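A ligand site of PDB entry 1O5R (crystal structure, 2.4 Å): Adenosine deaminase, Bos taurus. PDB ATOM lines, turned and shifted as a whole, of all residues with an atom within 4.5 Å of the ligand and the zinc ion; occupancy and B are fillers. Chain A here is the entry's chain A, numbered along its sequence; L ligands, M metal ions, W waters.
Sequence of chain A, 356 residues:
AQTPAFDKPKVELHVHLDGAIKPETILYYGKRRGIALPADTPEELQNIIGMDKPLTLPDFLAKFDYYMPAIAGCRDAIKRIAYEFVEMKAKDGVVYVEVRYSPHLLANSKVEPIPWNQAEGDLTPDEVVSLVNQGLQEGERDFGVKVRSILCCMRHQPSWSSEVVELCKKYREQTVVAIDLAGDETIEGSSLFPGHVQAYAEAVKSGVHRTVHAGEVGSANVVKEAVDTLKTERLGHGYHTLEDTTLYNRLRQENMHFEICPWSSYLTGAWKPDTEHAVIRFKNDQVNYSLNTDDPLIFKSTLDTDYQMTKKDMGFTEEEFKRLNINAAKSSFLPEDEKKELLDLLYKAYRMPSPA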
ATOM      1  N   HIS A  14     -11.969  10.279  30.782  1.00  0.00           N
ATOM      2  CA  HIS A  14     -13.009  10.506  29.791  1.00  0.00           C
ATOM      3  C   HIS A  14     -13.112   9.377  28.655  1.00  0.00           C
ATOM      4  O   HIS A  14     -12.396   9.457  27.635  1.00  0.00           O
ATOM      5  CB  HIS A  14     -13.070  11.792  28.947  1.00  0.00           C
ATOM      6  CG  HIS A  14     -14.231  12.275  28.120  1.00  0.00           C
ATOM      7  ND1 HIS A  14     -14.574  13.579  28.271  1.00  0.00           N
ATOM      8  CD2 HIS A  14     -15.212  11.649  27.332  1.00  0.00           C
ATOM      9  CE1 HIS A  14     -15.718  13.737  27.588  1.00  0.00           C
ATOM     10  NE2 HIS A  14     -16.125  12.602  27.016  1.00  0.00           N
ATOM     11  N   HIS A  16     -15.975   6.479  26.988  1.00  0.00           N
ATOM     12  CA  HIS A  16     -17.337   5.979  27.127  1.00  0.00           C
ATOM     13  C   HIS A  16     -17.556   4.451  27.025  1.00  0.00           C
ATOM     14  O   HIS A  16     -17.220   3.918  25.997  1.00  0.00           O
ATOM     15  CB  HIS A  16     -18.169   6.621  25.970  1.00  0.00           C
ATOM     16  CG  HIS A  16     -18.409   8.108  26.043  1.00  0.00           C
ATOM     17  ND1 HIS A  16     -19.571   8.610  26.485  1.00  0.00           N
ATOM     18  CD2 HIS A  16     -17.603   9.116  25.669  1.00  0.00           C
ATOM     19  CE1 HIS A  16     -19.457   9.984  26.349  1.00  0.00           C
ATOM     20  NE2 HIS A  16     -18.255  10.289  25.879  1.00  0.00           N
ATOM     21  N   ASP A  18     -20.125   2.351  26.349  1.00  0.00           N
ATOM     22  CA  ASP A  18     -20.740   1.937  25.079  1.00  0.00           C
ATOM     23  C   ASP A  18     -20.011   2.318  23.866  1.00  0.00           C
ATOM     24  O   ASP A  18     -20.412   2.163  22.778  1.00  0.00           O
ATOM     25  CB  ASP A  18     -22.184   2.433  25.130  1.00  0.00           C
ATOM     26  CG  ASP A  18     -22.345   3.948  25.137  1.00  0.00           C
ATOM     27  OD1 ASP A  18     -23.392   4.422  24.841  1.00  0.00           O
ATOM     28  OD2 ASP A  18     -21.436   4.666  25.408  1.00  0.00           O
ATOM     29  N   LEU A  55     -16.834  12.690  10.107  1.00  0.00           N
ATOM     30  CA  LEU A  55     -18.208  12.522   9.636  1.00  0.00           C
ATOM     31  C   LEU A  55     -19.142  13.548  10.265  1.00  0.00           C
ATOM     32  O   LEU A  55     -18.738  14.463  10.970  1.00  0.00           O
ATOM     33  CB  LEU A  55     -18.667  11.114  10.023  1.00  0.00           C
ATOM     34  CG  LEU A  55     -18.726  10.167   8.819  1.00  0.00           C
ATOM     35  CD1 LEU A  55     -17.460  10.219   7.958  1.00  0.00           C
ATOM     36  CD2 LEU A  55     -18.903   8.706   9.219  1.00  0.00           C
ATOM     37  N   THR A  56     -20.438  13.419   9.932  1.00  0.00           N
ATOM     38  CA  THR A  56     -21.453  14.269  10.533  1.00  0.00           C
ATOM     39  C   THR A  56     -22.237  13.537  11.618  1.00  0.00           C
ATOM     40  O   THR A  56     -22.239  12.315  11.710  1.00  0.00           O
ATOM     41  CB  THR A  56     -22.397  14.747   9.433  1.00  0.00           C
ATOM     42  OG1 THR A  56     -23.257  13.668   9.051  1.00  0.00           O
ATOM     43  CG2 THR A  56     -21.583  15.190   8.211  1.00  0.00           C
ATOM     44  N   LEU A  57     -22.898  14.327  12.487  1.00  0.00           N
ATOM     45  CA  LEU A  57     -23.637  13.737  13.587  1.00  0.00           C
ATOM     46  C   LEU A  57     -24.413  12.489  13.159  1.00  0.00           C
ATOM     47  O   LEU A  57     -24.232  11.389  13.670  1.00  0.00           O
ATOM     48  CB  LEU A  57     -24.606  14.781  14.139  1.00  0.00           C
ATOM     49  CG  LEU A  57     -25.089  14.444  15.557  1.00  0.00           C
ATOM     50  CD1 LEU A  57     -24.213  13.389  16.226  1.00  0.00           C
ATOM     51  CD2 LEU A  57     -25.082  15.655  16.489  1.00  0.00           C
ATOM     52  N   PHE A  60     -22.422   9.875  12.196  1.00  0.00           N
ATOM     53  CA  PHE A  60     -21.891   9.384  13.482  1.00  0.00           C
ATOM     54  C   PHE A  60     -22.795   8.542  14.382  1.00  0.00           C
ATOM     55  O   PHE A  60     -22.388   7.581  15.046  1.00  0.00           O
ATOM     56  CB  PHE A  60     -21.227  10.536  14.193  1.00  0.00           C
ATOM     57  CG  PHE A  60     -20.669  10.195  15.574  1.00  0.00           C
ATOM     58  CD1 PHE A  60     -19.291   9.943  15.680  1.00  0.00           C
ATOM     59  CD2 PHE A  60     -21.469  10.162  16.724  1.00  0.00           C
ATOM     60  CE1 PHE A  60     -18.714   9.633  16.930  1.00  0.00           C
ATOM     61  CE2 PHE A  60     -20.904   9.821  17.984  1.00  0.00           C
ATOM     62  CZ  PHE A  60     -19.536   9.516  18.081  1.00  0.00           C
ATOM     63  N   LEU A  61     -24.091   8.902  14.487  1.00  0.00           N
ATOM     64  CA  LEU A  61     -24.968   8.091  15.350  1.00  0.00           C
ATOM     65  C   LEU A  61     -25.482   6.796  14.823  1.00  0.00           C
ATOM     66  O   LEU A  61     -25.939   5.964  15.578  1.00  0.00           O
ATOM     67  CB  LEU A  61     -26.257   8.861  15.720  1.00  0.00           C
ATOM     68  CG  LEU A  61     -26.070  10.115  16.578  1.00  0.00           C
ATOM     69  CD1 LEU A  61     -27.369  10.950  16.499  1.00  0.00           C
ATOM     70  CD2 LEU A  61     -25.853   9.854  18.072  1.00  0.00           C
ATOM     71  N   PHE A  64     -23.733   3.572  16.235  1.00  0.00           N
ATOM     72  CA  PHE A  64     -24.327   2.902  17.403  1.00  0.00           C
ATOM     73  C   PHE A  64     -25.525   1.966  17.090  1.00  0.00           C
ATOM     74  O   PHE A  64     -25.773   0.916  17.729  1.00  0.00           O
ATOM     75  CB  PHE A  64     -24.844   3.928  18.514  1.00  0.00           C
ATOM     76  CG  PHE A  64     -23.749   4.757  19.195  1.00  0.00           C
ATOM     77  CD1 PHE A  64     -23.533   6.046  18.755  1.00  0.00           C
ATOM     78  CD2 PHE A  64     -23.000   4.221  20.290  1.00  0.00           C
ATOM     79  CE1 PHE A  64     -22.514   6.788  19.349  1.00  0.00           C
ATOM     80  CE2 PHE A  64     -21.956   4.980  20.850  1.00  0.00           C
ATOM     81  CZ  PHE A  64     -21.717   6.252  20.329  1.00  0.00           C
ATOM     82  N   ARG A 100     -17.452   6.217  31.506  1.00  0.00           N
ATOM     83  CA  ARG A 100     -18.789   6.790  31.537  1.00  0.00           C
ATOM     84  C   ARG A 100     -19.748   6.166  30.525  1.00  0.00           C
ATOM     85  O   ARG A 100     -19.365   5.651  29.488  1.00  0.00           O
ATOM     86  CB  ARG A 100     -18.672   8.298  31.314  1.00  0.00           C
ATOM     87  CG  ARG A 100     -18.822   8.714  29.846  1.00  0.00           C
ATOM     88  CD  ARG A 100     -18.519  10.200  29.719  1.00  0.00           C
ATOM     89  NE  ARG A 100     -18.204  10.720  31.060  1.00  0.00           N
ATOM     90  CZ  ARG A 100     -17.225  11.630  31.167  1.00  0.00           C
ATOM     91  NH1 ARG A 100     -16.713  12.187  30.080  1.00  0.00           N
ATOM     92  NH2 ARG A 100     -16.614  11.777  32.341  1.00  0.00           N
ATOM     93  N   TYR A 101     -21.038   6.198  30.908  1.00  0.00           N
ATOM     94  CA  TYR A 101     -22.061   5.621  30.041  1.00  0.00           C
ATOM     95  C   TYR A 101     -23.466   5.938  30.559  1.00  0.00           C
ATOM     96  O   TYR A 101     -23.672   6.284  31.720  1.00  0.00           O
ATOM     97  CB  TYR A 101     -21.845   4.105  30.014  1.00  0.00           C
ATOM     98  CG  TYR A 101     -22.231   3.517  31.329  1.00  0.00           C
ATOM     99  CD1 TYR A 101     -23.456   2.865  31.475  1.00  0.00           C
ATOM    100  CD2 TYR A 101     -21.340   3.570  32.405  1.00  0.00           C
ATOM    101  CE1 TYR A 101     -23.778   2.252  32.674  1.00  0.00           C
ATOM    102  CE2 TYR A 101     -21.670   2.951  33.608  1.00  0.00           C
ATOM    103  CZ  TYR A 101     -22.879   2.309  33.746  1.00  0.00           C
ATOM    104  OH  TYR A 101     -23.220   1.708  34.950  1.00  0.00           O
ATOM    105  N   SER A 102     -24.440   5.838  29.650  1.00  0.00           N
ATOM    106  CA  SER A 102     -25.825   6.080  30.055  1.00  0.00           C
ATOM    107  C   SER A 102     -26.581   4.760  30.278  1.00  0.00           C
ATOM    108  O   SER A 102     -26.756   3.947  29.386  1.00  0.00           O
ATOM    109  CB  SER A 102     -26.498   6.885  28.942  1.00  0.00           C
ATOM    110  OG  SER A 102     -27.863   7.118  29.298  1.00  0.00           O
ATOM    111  N   LEU A 105     -29.631   3.886  28.027  1.00  0.00           N
ATOM    112  CA  LEU A 105     -29.391   3.467  26.649  1.00  0.00           C
ATOM    113  C   LEU A 105     -29.008   1.986  26.566  1.00  0.00           C
ATOM    114  O   LEU A 105     -28.950   1.381  25.501  1.00  0.00           O
ATOM    115  CB  LEU A 105     -28.286   4.341  26.058  1.00  0.00           C
ATOM    116  CG  LEU A 105     -28.747   5.775  25.778  1.00  0.00           C
ATOM    117  CD1 LEU A 105     -27.665   6.617  25.093  1.00  0.00           C
ATOM    118  CD2 LEU A 105     -29.964   5.832  24.858  1.00  0.00           C
ATOM    119  N   MET A 154     -28.584  12.387  29.481  1.00  0.00           N
ATOM    120  CA  MET A 154     -28.667  12.642  28.048  1.00  0.00           C
ATOM    121  C   MET A 154     -29.353  13.976  27.749  1.00  0.00           C
ATOM    122  O   MET A 154     -30.436  14.280  28.205  1.00  0.00           O
ATOM    123  CB  MET A 154     -29.437  11.481  27.399  1.00  0.00           C
ATOM    124  CG  MET A 154     -28.629  10.180  27.378  1.00  0.00           C
ATOM    125  SD  MET A 154     -27.002  10.396  26.638  1.00  0.00           S
ATOM    126  CE  MET A 154     -27.550  10.736  24.952  1.00  0.00           C
ATOM    127  N   HIS A 156     -30.907  15.285  25.326  1.00  0.00           N
ATOM    128  CA  HIS A 156     -32.226  15.358  24.699  1.00  0.00           C
ATOM    129  C   HIS A 156     -33.330  14.681  25.527  1.00  0.00           C
ATOM    130  O   HIS A 156     -34.467  14.536  25.106  1.00  0.00           O
ATOM    131  CB  HIS A 156     -32.139  14.696  23.320  1.00  0.00           C
ATOM    132  CG  HIS A 156     -31.817  13.233  23.483  1.00  0.00           C
ATOM    133  ND1 HIS A 156     -30.594  12.780  23.830  1.00  0.00           N
ATOM    134  CD2 HIS A 156     -32.684  12.146  23.375  1.00  0.00           C
ATOM    135  CE1 HIS A 156     -30.719  11.437  23.932  1.00  0.00           C
ATOM    136  NE2 HIS A 156     -31.961  11.033  23.668  1.00  0.00           N
ATOM    137  N   GLY A 183     -25.224  13.517  24.885  1.00  0.00           N
ATOM    138  CA  GLY A 183     -24.385  14.449  24.156  1.00  0.00           C
ATOM    139  C   GLY A 183     -25.206  15.342  23.224  1.00  0.00           C
ATOM    140  O   GLY A 183     -26.373  15.632  23.454  1.00  0.00           O
ATOM    141  N   ASP A 184     -24.541  15.815  22.159  1.00  0.00           N
ATOM    142  CA  ASP A 184     -25.236  16.735  21.262  1.00  0.00           C
ATOM    143  C   ASP A 184     -25.586  18.036  21.987  1.00  0.00           C
ATOM    144  O   ASP A 184     -26.737  18.317  22.321  1.00  0.00           O
ATOM    145  CB  ASP A 184     -26.524  16.046  20.791  1.00  0.00           C
ATOM    146  CG  ASP A 184     -27.109  16.836  19.627  1.00  0.00           C
ATOM    147  OD1 ASP A 184     -26.604  17.926  19.373  1.00  0.00           O
ATOM    148  OD2 ASP A 184     -28.046  16.357  18.993  1.00  0.00           O
ATOM    149  N   HIS A 213     -20.146  17.559  29.389  1.00  0.00           N
ATOM    150  CA  HIS A 213     -19.722  17.707  28.002  1.00  0.00           C
ATOM    151  C   HIS A 213     -20.066  19.107  27.491  1.00  0.00           C
ATOM    152  O   HIS A 213     -21.224  19.441  27.259  1.00  0.00           O
ATOM    153  CB  HIS A 213     -20.458  16.671  27.159  1.00  0.00           C
ATOM    154  CG  HIS A 213     -19.672  15.381  27.134  1.00  0.00           C
ATOM    155  ND1 HIS A 213     -19.850  14.393  28.028  1.00  0.00           N
ATOM    156  CD2 HIS A 213     -18.762  14.945  26.159  1.00  0.00           C
ATOM    157  CE1 HIS A 213     -19.077  13.375  27.608  1.00  0.00           C
ATOM    158  NE2 HIS A 213     -18.410  13.677  26.484  1.00  0.00           N
ATOM    159  N   GLU A 216     -17.230  21.159  23.121  1.00  0.00           N
ATOM    160  CA  GLU A 216     -16.677  20.278  22.091  1.00  0.00           C
ATOM    161  C   GLU A 216     -17.091  20.741  20.691  1.00  0.00           C
ATOM    162  O   GLU A 216     -16.276  20.967  19.806  1.00  0.00           O
ATOM    163  CB  GLU A 216     -17.172  18.855  22.353  1.00  0.00           C
ATOM    164  CG  GLU A 216     -16.913  17.923  21.170  1.00  0.00           C
ATOM    165  CD  GLU A 216     -17.512  16.565  21.460  1.00  0.00           C
ATOM    166  OE1 GLU A 216     -18.286  16.454  22.398  1.00  0.00           O
ATOM    167  OE2 GLU A 216     -17.191  15.620  20.742  1.00  0.00           O
ATOM    168  N   HIS A 237     -13.910  18.188  27.191  1.00  0.00           N
ATOM    169  CA  HIS A 237     -13.427  18.919  26.032  1.00  0.00           C
ATOM    170  C   HIS A 237     -13.153  20.384  26.383  1.00  0.00           C
ATOM    171  O   HIS A 237     -12.028  20.802  26.603  1.00  0.00           O
ATOM    172  CB  HIS A 237     -14.512  18.844  24.945  1.00  0.00           C
ATOM    173  CG  HIS A 237     -14.683  17.424  24.495  1.00  0.00           C
ATOM    174  ND1 HIS A 237     -13.816  16.789  23.677  1.00  0.00           N
ATOM    175  CD2 HIS A 237     -15.762  16.562  24.752  1.00  0.00           C
ATOM    176  CE1 HIS A 237     -14.353  15.581  23.435  1.00  0.00           C
ATOM    177  NE2 HIS A 237     -15.518  15.417  24.062  1.00  0.00           N
ATOM    178  N   THR A 268     -14.522  14.010  14.744  1.00  0.00           N
ATOM    179  CA  THR A 268     -15.788  14.700  14.892  1.00  0.00           C
ATOM    180  C   THR A 268     -15.974  16.009  14.165  1.00  0.00           C
ATOM    181  O   THR A 268     -17.069  16.508  14.152  1.00  0.00           O
ATOM    182  CB  THR A 268     -16.240  14.977  16.305  1.00  0.00           C
ATOM    183  OG1 THR A 268     -15.402  15.972  16.903  1.00  0.00           O
ATOM    184  CG2 THR A 268     -16.308  13.744  17.135  1.00  0.00           C
ATOM    185  N   ASP A 294     -12.147   8.805  24.557  1.00  0.00           N
ATOM    186  CA  ASP A 294     -13.521   9.047  24.257  1.00  0.00           C
ATOM    187  C   ASP A 294     -14.186   7.795  23.843  1.00  0.00           C
ATOM    188  O   ASP A 294     -14.970   7.178  24.543  1.00  0.00           O
ATOM    189  CB  ASP A 294     -13.688  10.262  23.334  1.00  0.00           C
ATOM    190  CG  ASP A 294     -14.909  11.208  23.381  1.00  0.00           C
ATOM    191  OD1 ASP A 294     -15.140  12.022  22.460  1.00  0.00           O
ATOM    192  OD2 ASP A 294     -15.543  11.117  24.426  1.00  0.00           O
ATOM    193  N   ASP A 295     -13.823   7.394  22.644  1.00  0.00           N
ATOM    194  CA  ASP A 295     -14.465   6.224  22.067  1.00  0.00           C
ATOM    195  C   ASP A 295     -13.471   5.407  21.275  1.00  0.00           C
ATOM    196  O   ASP A 295     -13.407   5.528  20.057  1.00  0.00           O
ATOM    197  CB  ASP A 295     -15.613   6.468  21.059  1.00  0.00           C
ATOM    198  CG  ASP A 295     -16.790   7.242  21.699  1.00  0.00           C
ATOM    199  OD1 ASP A 295     -17.868   6.688  22.099  1.00  0.00           O
ATOM    200  OD2 ASP A 295     -16.677   8.449  21.795  1.00  0.00           O
ATOM    201  N   PHE A 299     -13.693   5.223  17.119  1.00  0.00           N
ATOM    202  CA  PHE A 299     -12.549   5.928  16.412  1.00  0.00           C
ATOM    203  C   PHE A 299     -11.249   5.100  15.961  1.00  0.00           C
ATOM    204  O   PHE A 299     -10.202   5.634  15.792  1.00  0.00           O
ATOM    205  CB  PHE A 299     -12.122   7.126  17.299  1.00  0.00           C
ATOM    206  CG  PHE A 299     -13.227   8.066  17.638  1.00  0.00           C
ATOM    207  CD1 PHE A 299     -14.212   8.428  16.702  1.00  0.00           C
ATOM    208  CD2 PHE A 299     -13.270   8.594  18.958  1.00  0.00           C
ATOM    209  CE1 PHE A 299     -15.286   9.264  17.132  1.00  0.00           C
ATOM    210  CE2 PHE A 299     -14.366   9.428  19.419  1.00  0.00           C
ATOM    211  CZ  PHE A 299     -15.381   9.736  18.481  1.00  0.00           C
HETATM  212  C1  LIG L   1     -21.445   9.888  23.312  1.00  0.00           C
HETATM  213  N1  LIG L   1     -21.738   8.496  23.721  1.00  0.00           N
HETATM  214  C2  LIG L   1     -20.728   7.838  23.177  1.00  0.00           C
HETATM  215  N2  LIG L   1     -19.826   8.556  22.568  1.00  0.00           N
HETATM  216  C3  LIG L   1     -20.268   9.944  22.644  1.00  0.00           C
HETATM  217  C4  LIG L   1     -19.494  11.070  22.145  1.00  0.00           C
HETATM  218  O1  LIG L   1     -19.971  12.057  22.342  1.00  0.00           O
HETATM  219  N3  LIG L   1     -18.485  10.875  21.461  1.00  0.00           N
HETATM  220  C5  LIG L   1     -22.951   7.920  24.293  1.00  0.00           C
HETATM  221  C6  LIG L   1     -22.957   7.803  25.855  1.00  0.00           C
HETATM  222  O2  LIG L   1     -21.866   7.161  26.669  1.00  0.00           O
HETATM  223  C7  LIG L   1     -24.173   8.694  23.861  1.00  0.00           C
HETATM  224  C8  LIG L   1     -24.669   8.254  22.488  1.00  0.00           C
HETATM  225  N4  LIG L   1     -25.621   9.217  21.991  1.00  0.00           N
HETATM  226  C9  LIG L   1     -26.987   9.027  21.995  1.00  0.00           C
HETATM  227  C10 LIG L   1     -27.606  10.153  21.533  1.00  0.00           C
HETATM  228  C11 LIG L   1     -26.549  11.052  21.225  1.00  0.00           C
HETATM  229  C12 LIG L   1     -25.331  10.412  21.528  1.00  0.00           C
HETATM  230  C13 LIG L   1     -26.531  12.299  20.660  1.00  0.00           C
HETATM  231  C14 LIG L   1     -25.307  12.931  20.431  1.00  0.00           C
HETATM  232  C15 LIG L   1     -24.123  12.279  20.781  1.00  0.00           C
HETATM  233  C16 LIG L   1     -24.171  11.016  21.317  1.00  0.00           C
HETATM  234  N5  LIG L   1     -22.914  12.706  20.516  1.00  0.00           N
HETATM  235  C17 LIG L   1     -22.561  13.958  20.128  1.00  0.00           C
HETATM  236  O3  LIG L   1     -23.393  14.741  19.757  1.00  0.00           O
HETATM  237  N6  LIG L   1     -21.287  14.046  19.927  1.00  0.00           N
HETATM  238  C18 LIG L   1     -20.711  15.200  19.290  1.00  0.00           C
HETATM  239  C19 LIG L   1     -19.888  13.552  17.564  1.00  0.00           C
HETATM  240  C20 LIG L   1     -20.373  14.809  17.861  1.00  0.00           C
HETATM  241  C21 LIG L   1     -20.529  15.732  16.842  1.00  0.00           C
HETATM  242  C22 LIG L   1     -20.254  15.366  15.529  1.00  0.00           C
HETATM  243  C23 LIG L   1     -19.785  14.078  15.210  1.00  0.00           C
HETATM  244  C24 LIG L   1     -19.569  13.236  16.249  1.00  0.00           C
HETATM  245 ZN    ZN M   1     -17.418  11.983  25.490  1.00  0.00          ZN
HETATM  246  O   HOH W   1     -19.646  14.393  22.888  1.00  0.00           O
HETATM  247  O   HOH W   2     -17.665  13.194  20.384  1.00  0.00           O
HETATM  248  O   HOH W   3     -28.480  14.162  22.710  1.00  0.00           O
HETATM  249  O   HOH W   4     -17.350  12.704  23.839  1.00  0.00           O
HETATM  250  O   HOH W   5     -22.419  17.330  21.263  1.00  0.00           O
HETATM  251  O   HOH W   6     -23.470  17.638  18.355  1.00  0.00           O
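OD2 of Asp 18 lies within hydrogen-bond range of O2 of the ligand (2.8 Å).
N2 of the ligand sits at hydrogen-bond distance from OD1 of Asp 295, at 2.7 Å.
A ring nitrogen (ND1) of His 16 is in hydrogen-bond range of an oxygen (O2) of the ligand, 2.7 Å away.
The backbone NH (N) of Asp 184 is in hydrogen-bond range of an oxygen (O3) of the ligand (2.9 Å).
NH1 of Arg 100 sits close to ND1 of His 14.
A ring nitrogen (NE2) of His 237 is in hydrogen-bond range of the side-chain carboxylate (OE1) of Glu 216, at 3.4 Å.
Merely in contact with the ligand: Leu 57, Phe 60, Leu 61, Phe 64, Tyr 101, Leu 105, Met 154, Gly 183, Glu 216 and Thr 268.
Hydrophobic or aromatic side chains within 4 Å of the ligand: His 16, Leu 57, Phe 60, Leu 61, Phe 64, Leu 105 and Met 154.
Of the 24 residues printed, 15 come within 4 Å of the ligand.
Four residues have an atom within 4 Å of the zinc ion: His 14, His 16, His 213 and Asp 294.
The nearest printed residue that does not touch the zinc ion is His 237 (4.2 Å).
Water W4 is bound to the zinc ion, 1.8 Å away.
The zinc ion is bound by NE2 of His 16.
NE2 of His 14 is bound to the zinc ion (2.1 Å).
The zinc ion is bound by NE2 of His 213 (2.2 Å).
OD2 of Asp 294 binds the zinc ion (2.3 Å).
The zinc ion has five donor atoms within binding distance.
Water W4 lies within hydrogen-bond range of the side-chain carboxylate of Asp 294 (2.7 Å), an oxygen (O1) of the ligand (3.1 Å) and a ring nitrogen (NE2) of His 237 (3.3 Å).
Water W1 bridges an oxygen (O1) of the ligand and the side-chain carboxylate of Glu 216.
Water W2 lies within hydrogen-bond range of OE2 of Glu 216 (2.5 Å), N3 of the ligand (2.7 Å) and OD1 of Asp 294 (3.5 Å).
Water W5 bridges the backbone NH (N) of Asp 184 and an oxygen (O3) of the ligand.
Water W6 bridges an oxygen (O3) of the ligand and the side-chain carboxylate of Asp 184.
Water W3 lies within hydrogen-bond range of the backbone carbonyl oxygen of Gly 183 (2.7 Å) and a ring nitrogen (ND1) of His 156 (2.8 Å).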
